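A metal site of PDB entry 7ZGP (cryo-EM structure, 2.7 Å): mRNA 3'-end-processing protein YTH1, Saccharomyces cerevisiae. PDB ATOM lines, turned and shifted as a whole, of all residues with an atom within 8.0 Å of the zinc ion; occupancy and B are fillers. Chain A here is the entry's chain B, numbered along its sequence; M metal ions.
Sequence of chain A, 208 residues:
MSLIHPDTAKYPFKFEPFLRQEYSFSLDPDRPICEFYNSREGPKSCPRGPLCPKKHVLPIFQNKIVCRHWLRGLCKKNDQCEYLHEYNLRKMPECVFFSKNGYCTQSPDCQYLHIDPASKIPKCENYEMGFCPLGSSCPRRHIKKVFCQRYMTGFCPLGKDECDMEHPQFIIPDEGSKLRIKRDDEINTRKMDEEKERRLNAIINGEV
The backbone NH of Lys 54 lies close to the side-chain sulfur of Cys 52 (3.4 Å). The side-chain sulfur of Cys 34 sits close to the backbone NH of Phe 36, 3.6 Å away. N of Tyr 37 sits close to SG of Cys 34 (3.4 Å). SG of Cys 52 sits close to NE of Arg 48. The backbone carbonyl oxygen (O) of Lys 55 sits at hydrogen-bond distance from the backbone NH (N) of Cys 34 (3.2 Å). SG of Cys 46 lies close to N of Arg 48 (3.6 Å).
The zinc ion is bound by a ring nitrogen (NE2) of His 56 (2.1 Å), the side-chain sulfur (SG) of Cys 46 (2.3 Å), the side-chain sulfur (SG) of Cys 52 (2.3 Å) and the side-chain sulfur (SG) of Cys 34 (2.3 Å).
Within 4 Å of the zinc ion: Cys 34, Cys 46, Cys 52 and His 56. The nearest printed residue that does not touch the zinc ion is Arg 48 (4.2 Å).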
ATOM      1  N   PRO A  32     -12.991  -6.728   3.814  1.00  0.00           N
ATOM      2  CA  PRO A  32     -13.850  -7.296   2.766  1.00  0.00           C
ATOM      3  C   PRO A  32     -14.034  -8.795   2.950  1.00  0.00           C
ATOM      4  O   PRO A  32     -13.162  -9.494   3.471  1.00  0.00           O
ATOM      5  CB  PRO A  32     -13.107  -6.967   1.475  1.00  0.00           C
ATOM      6  CG  PRO A  32     -11.700  -6.697   1.880  1.00  0.00           C
ATOM      7  CD  PRO A  32     -11.774  -6.113   3.250  1.00  0.00           C
ATOM      8  N   ILE A  33     -15.192  -9.287   2.510  1.00  0.00           N
ATOM      9  CA  ILE A  33     -15.494 -10.705   2.616  1.00  0.00           C
ATOM     10  C   ILE A  33     -14.598 -11.489   1.663  1.00  0.00           C
ATOM     11  O   ILE A  33     -14.127 -10.963   0.642  1.00  0.00           O
ATOM     12  CB  ILE A  33     -16.982 -10.969   2.334  1.00  0.00           C
ATOM     13  CG1 ILE A  33     -17.536 -11.995   3.311  1.00  0.00           C
ATOM     14  CG2 ILE A  33     -17.207 -11.405   0.894  1.00  0.00           C
ATOM     15  CD1 ILE A  33     -17.568 -11.517   4.744  1.00  0.00           C
ATOM     16  N   CYS A  34     -14.347 -12.755   1.994  1.00  0.00           N
ATOM     17  CA  CYS A  34     -13.509 -13.585   1.147  1.00  0.00           C
ATOM     18  C   CYS A  34     -14.255 -13.992  -0.112  1.00  0.00           C
ATOM     19  O   CYS A  34     -15.386 -14.479  -0.043  1.00  0.00           O
ATOM     20  CB  CYS A  34     -13.030 -14.817   1.910  1.00  0.00           C
ATOM     21  SG  CYS A  34     -11.689 -15.718   1.102  1.00  0.00           S
ATOM     22  N   GLU A  35     -13.611 -13.817  -1.267  1.00  0.00           N
ATOM     23  CA  GLU A  35     -14.206 -14.185  -2.535  1.00  0.00           C
ATOM     24  C   GLU A  35     -14.068 -15.671  -2.849  1.00  0.00           C
ATOM     25  O   GLU A  35     -14.703 -16.147  -3.795  1.00  0.00           O
ATOM     26  CB  GLU A  35     -13.595 -13.364  -3.691  1.00  0.00           C
ATOM     27  CG  GLU A  35     -12.057 -13.414  -3.868  1.00  0.00           C
ATOM     28  CD  GLU A  35     -11.225 -12.871  -2.709  1.00  0.00           C
ATOM     29  OE1 GLU A  35     -10.052 -12.542  -2.941  1.00  0.00           O
ATOM     30  OE2 GLU A  35     -11.735 -12.750  -1.576  1.00  0.00           O
ATOM     31  N   PHE A  36     -13.269 -16.403  -2.080  1.00  0.00           N
ATOM     32  CA  PHE A  36     -13.063 -17.826  -2.297  1.00  0.00           C
ATOM     33  C   PHE A  36     -13.654 -18.697  -1.200  1.00  0.00           C
ATOM     34  O   PHE A  36     -14.096 -19.814  -1.486  1.00  0.00           O
ATOM     35  CB  PHE A  36     -11.571 -18.137  -2.420  1.00  0.00           C
ATOM     36  CG  PHE A  36     -10.862 -17.332  -3.465  1.00  0.00           C
ATOM     37  CD1 PHE A  36     -11.449 -17.095  -4.691  1.00  0.00           C
ATOM     38  CD2 PHE A  36      -9.605 -16.805  -3.222  1.00  0.00           C
ATOM     39  CE1 PHE A  36     -10.801 -16.355  -5.666  1.00  0.00           C
ATOM     40  CE2 PHE A  36      -8.948 -16.064  -4.176  1.00  0.00           C
ATOM     41  CZ  PHE A  36      -9.549 -15.832  -5.400  1.00  0.00           C
ATOM     42  N   TYR A  37     -13.670 -18.224   0.037  1.00  0.00           N
ATOM     43  CA  TYR A  37     -14.138 -19.036   1.151  1.00  0.00           C
ATOM     44  C   TYR A  37     -15.622 -19.338   1.026  1.00  0.00           C
ATOM     45  O   TYR A  37     -16.419 -18.477   0.636  1.00  0.00           O
ATOM     46  CB  TYR A  37     -13.849 -18.340   2.485  1.00  0.00           C
ATOM     47  CG  TYR A  37     -14.223 -19.157   3.696  1.00  0.00           C
ATOM     48  CD1 TYR A  37     -13.349 -20.100   4.215  1.00  0.00           C
ATOM     49  CD2 TYR A  37     -15.442 -18.983   4.332  1.00  0.00           C
ATOM     50  CE1 TYR A  37     -13.684 -20.861   5.327  1.00  0.00           C
ATOM     51  CE2 TYR A  37     -15.791 -19.727   5.439  1.00  0.00           C
ATOM     52  CZ  TYR A  37     -14.899 -20.662   5.935  1.00  0.00           C
ATOM     53  OH  TYR A  37     -15.239 -21.413   7.034  1.00  0.00           O
ATOM     54  N   ASN A  38     -15.994 -20.566   1.356  1.00  0.00           N
ATOM     55  CA  ASN A  38     -17.382 -20.995   1.394  1.00  0.00           C
ATOM     56  C   ASN A  38     -17.610 -21.661   2.741  1.00  0.00           C
ATOM     57  O   ASN A  38     -16.873 -22.591   3.108  1.00  0.00           O
ATOM     58  CB  ASN A  38     -17.701 -21.934   0.204  1.00  0.00           C
ATOM     59  CG  ASN A  38     -18.970 -22.767   0.393  1.00  0.00           C
ATOM     60  OD1 ASN A  38     -19.173 -23.437   1.408  1.00  0.00           O
ATOM     61  ND2 ASN A  38     -19.845 -22.704  -0.599  1.00  0.00           N
ATOM     62  N   PRO A  43     -12.916 -24.734   5.844  1.00  0.00           N
ATOM     63  CA  PRO A  43     -11.710 -23.896   5.725  1.00  0.00           C
ATOM     64  C   PRO A  43     -10.848 -24.239   4.528  1.00  0.00           C
ATOM     65  O   PRO A  43     -10.079 -23.377   4.071  1.00  0.00           O
ATOM     66  CB  PRO A  43     -10.962 -24.160   7.045  1.00  0.00           C
ATOM     67  CG  PRO A  43     -12.009 -24.697   7.974  1.00  0.00           C
ATOM     68  CD  PRO A  43     -12.963 -25.463   7.118  1.00  0.00           C
ATOM     69  N   SER A  45     -11.677 -24.538   1.527  1.00  0.00           N
ATOM     70  CA  SER A  45     -12.124 -23.915   0.286  1.00  0.00           C
ATOM     71  C   SER A  45     -11.277 -22.691  -0.056  1.00  0.00           C
ATOM     72  O   SER A  45     -11.093 -22.367  -1.231  1.00  0.00           O
ATOM     73  CB  SER A  45     -13.595 -23.537   0.399  1.00  0.00           C
ATOM     74  OG  SER A  45     -13.747 -22.195   0.829  1.00  0.00           O
ATOM     75  N   CYS A  46     -10.775 -21.994   0.958  1.00  0.00           N
ATOM     76  CA  CYS A  46      -9.950 -20.809   0.721  1.00  0.00           C
ATOM     77  C   CYS A  46      -8.516 -21.234   0.422  1.00  0.00           C
ATOM     78  O   CYS A  46      -7.902 -21.917   1.246  1.00  0.00           O
ATOM     79  CB  CYS A  46      -9.984 -19.889   1.931  1.00  0.00           C
ATOM     80  SG  CYS A  46      -8.968 -18.401   1.755  1.00  0.00           S
ATOM     81  N   PRO A  47      -7.949 -20.860  -0.730  1.00  0.00           N
ATOM     82  CA  PRO A  47      -6.549 -21.226  -1.004  1.00  0.00           C
ATOM     83  C   PRO A  47      -5.559 -20.656  -0.007  1.00  0.00           C
ATOM     84  O   PRO A  47      -4.562 -21.314   0.306  1.00  0.00           O
ATOM     85  CB  PRO A  47      -6.321 -20.658  -2.416  1.00  0.00           C
ATOM     86  CG  PRO A  47      -7.329 -19.564  -2.545  1.00  0.00           C
ATOM     87  CD  PRO A  47      -8.529 -20.031  -1.794  1.00  0.00           C
ATOM     88  N   ARG A  48      -5.815 -19.448   0.501  1.00  0.00           N
ATOM     89  CA  ARG A  48      -4.890 -18.817   1.437  1.00  0.00           C
ATOM     90  C   ARG A  48      -4.926 -19.462   2.823  1.00  0.00           C
ATOM     91  O   ARG A  48      -4.076 -19.134   3.659  1.00  0.00           O
ATOM     92  CB  ARG A  48      -5.183 -17.325   1.549  1.00  0.00           C
ATOM     93  CG  ARG A  48      -5.020 -16.567   0.248  1.00  0.00           C
ATOM     94  CD  ARG A  48      -5.579 -15.156   0.348  1.00  0.00           C
ATOM     95  NE  ARG A  48      -6.942 -15.072  -0.190  1.00  0.00           N
ATOM     96  CZ  ARG A  48      -7.449 -13.988  -0.755  1.00  0.00           C
ATOM     97  NH1 ARG A  48      -6.748 -12.875  -0.890  1.00  0.00           N
ATOM     98  NH2 ARG A  48      -8.701 -14.024  -1.204  1.00  0.00           N
ATOM     99  N   GLY A  49      -5.877 -20.349   3.085  1.00  0.00           N
ATOM    100  CA  GLY A  49      -5.961 -21.014   4.361  1.00  0.00           C
ATOM    101  C   GLY A  49      -6.469 -20.101   5.461  1.00  0.00           C
ATOM    102  O   GLY A  49      -7.018 -19.036   5.204  1.00  0.00           O
ATOM    103  N   PRO A  50      -6.288 -20.523   6.712  1.00  0.00           N
ATOM    104  CA  PRO A  50      -6.730 -19.678   7.844  1.00  0.00           C
ATOM    105  C   PRO A  50      -6.048 -18.323   7.888  1.00  0.00           C
ATOM    106  O   PRO A  50      -6.592 -17.387   8.481  1.00  0.00           O
ATOM    107  CB  PRO A  50      -6.384 -20.532   9.068  1.00  0.00           C
ATOM    108  CG  PRO A  50      -6.332 -21.926   8.569  1.00  0.00           C
ATOM    109  CD  PRO A  50      -5.799 -21.835   7.166  1.00  0.00           C
ATOM    110  N   LEU A  51      -4.856 -18.198   7.289  1.00  0.00           N
ATOM    111  CA  LEU A  51      -4.148 -16.923   7.295  1.00  0.00           C
ATOM    112  C   LEU A  51      -4.594 -16.051   6.126  1.00  0.00           C
ATOM    113  O   LEU A  51      -3.753 -15.549   5.370  1.00  0.00           O
ATOM    114  CB  LEU A  51      -2.632 -17.162   7.224  1.00  0.00           C
ATOM    115  CG  LEU A  51      -1.885 -17.381   8.541  1.00  0.00           C
ATOM    116  CD1 LEU A  51      -2.104 -16.215   9.489  1.00  0.00           C
ATOM    117  CD2 LEU A  51      -2.266 -18.698   9.189  1.00  0.00           C
ATOM    118  N   CYS A  52      -5.901 -15.859   5.985  1.00  0.00           N
ATOM    119  CA  CYS A  52      -6.414 -15.034   4.902  1.00  0.00           C
ATOM    120  C   CYS A  52      -6.756 -13.646   5.408  1.00  0.00           C
ATOM    121  O   CYS A  52      -7.436 -13.517   6.442  1.00  0.00           O
ATOM    122  CB  CYS A  52      -7.655 -15.673   4.285  1.00  0.00           C
ATOM    123  SG  CYS A  52      -8.383 -14.760   2.902  1.00  0.00           S
ATOM    124  N   PRO A  53      -6.309 -12.587   4.732  1.00  0.00           N
ATOM    125  CA  PRO A  53      -6.654 -11.225   5.184  1.00  0.00           C
ATOM    126  C   PRO A  53      -8.144 -10.925   5.112  1.00  0.00           C
ATOM    127  O   PRO A  53      -8.607 -10.005   5.784  1.00  0.00           O
ATOM    128  CB  PRO A  53      -5.854 -10.334   4.230  1.00  0.00           C
ATOM    129  CG  PRO A  53      -5.693 -11.150   3.001  1.00  0.00           C
ATOM    130  CD  PRO A  53      -5.533 -12.571   3.481  1.00  0.00           C
ATOM    131  N   LYS A  54      -8.901 -11.676   4.317  1.00  0.00           N
ATOM    132  CA  LYS A  54     -10.326 -11.435   4.149  1.00  0.00           C
ATOM    133  C   LYS A  54     -11.082 -12.051   5.336  1.00  0.00           C
ATOM    134  O   LYS A  54     -10.485 -12.524   6.308  1.00  0.00           O
ATOM    135  CB  LYS A  54     -10.798 -11.996   2.815  1.00  0.00           C
ATOM    136  CG  LYS A  54     -10.053 -11.458   1.619  1.00  0.00           C
ATOM    137  CD  LYS A  54     -10.351  -9.989   1.394  1.00  0.00           C
ATOM    138  CE  LYS A  54      -9.675  -9.481   0.132  1.00  0.00           C
ATOM    139  NZ  LYS A  54     -10.319 -10.042  -1.090  1.00  0.00           N
ATOM    140  N   LYS A  55     -12.416 -12.009   5.228  1.00  0.00           N
ATOM    141  CA  LYS A  55     -13.274 -12.506   6.337  1.00  0.00           C
ATOM    142  C   LYS A  55     -13.828 -13.892   6.002  1.00  0.00           C
ATOM    143  O   LYS A  55     -14.436 -14.049   4.932  1.00  0.00           O
ATOM    144  CB  LYS A  55     -14.403 -11.503   6.608  1.00  0.00           C
ATOM    145  CG  LYS A  55     -15.284 -11.852   7.798  1.00  0.00           C
ATOM    146  CD  LYS A  55     -16.120 -10.688   8.288  1.00  0.00           C
ATOM    147  CE  LYS A  55     -15.283  -9.559   8.849  1.00  0.00           C
ATOM    148  NZ  LYS A  55     -16.116  -8.544   9.549  1.00  0.00           N
ATOM    149  N   HIS A  56     -13.623 -14.847   6.909  1.00  0.00           N
ATOM    150  CA  HIS A  56     -14.139 -16.208   6.765  1.00  0.00           C
ATOM    151  C   HIS A  56     -15.306 -16.354   7.735  1.00  0.00           C
ATOM    152  O   HIS A  56     -15.127 -16.683   8.907  1.00  0.00           O
ATOM    153  CB  HIS A  56     -13.049 -17.243   7.044  1.00  0.00           C
ATOM    154  CG  HIS A  56     -12.021 -17.346   5.967  1.00  0.00           C
ATOM    155  ND1 HIS A  56     -10.987 -18.259   6.012  1.00  0.00           N
ATOM    156  CD2 HIS A  56     -11.863 -16.647   4.818  1.00  0.00           C
ATOM    157  CE1 HIS A  56     -10.234 -18.116   4.931  1.00  0.00           C
ATOM    158  NE2 HIS A  56     -10.746 -17.148   4.192  1.00  0.00           N
HETATM  159 ZN    ZN M   1      -9.934 -16.417   2.451  1.00  0.00          ZN
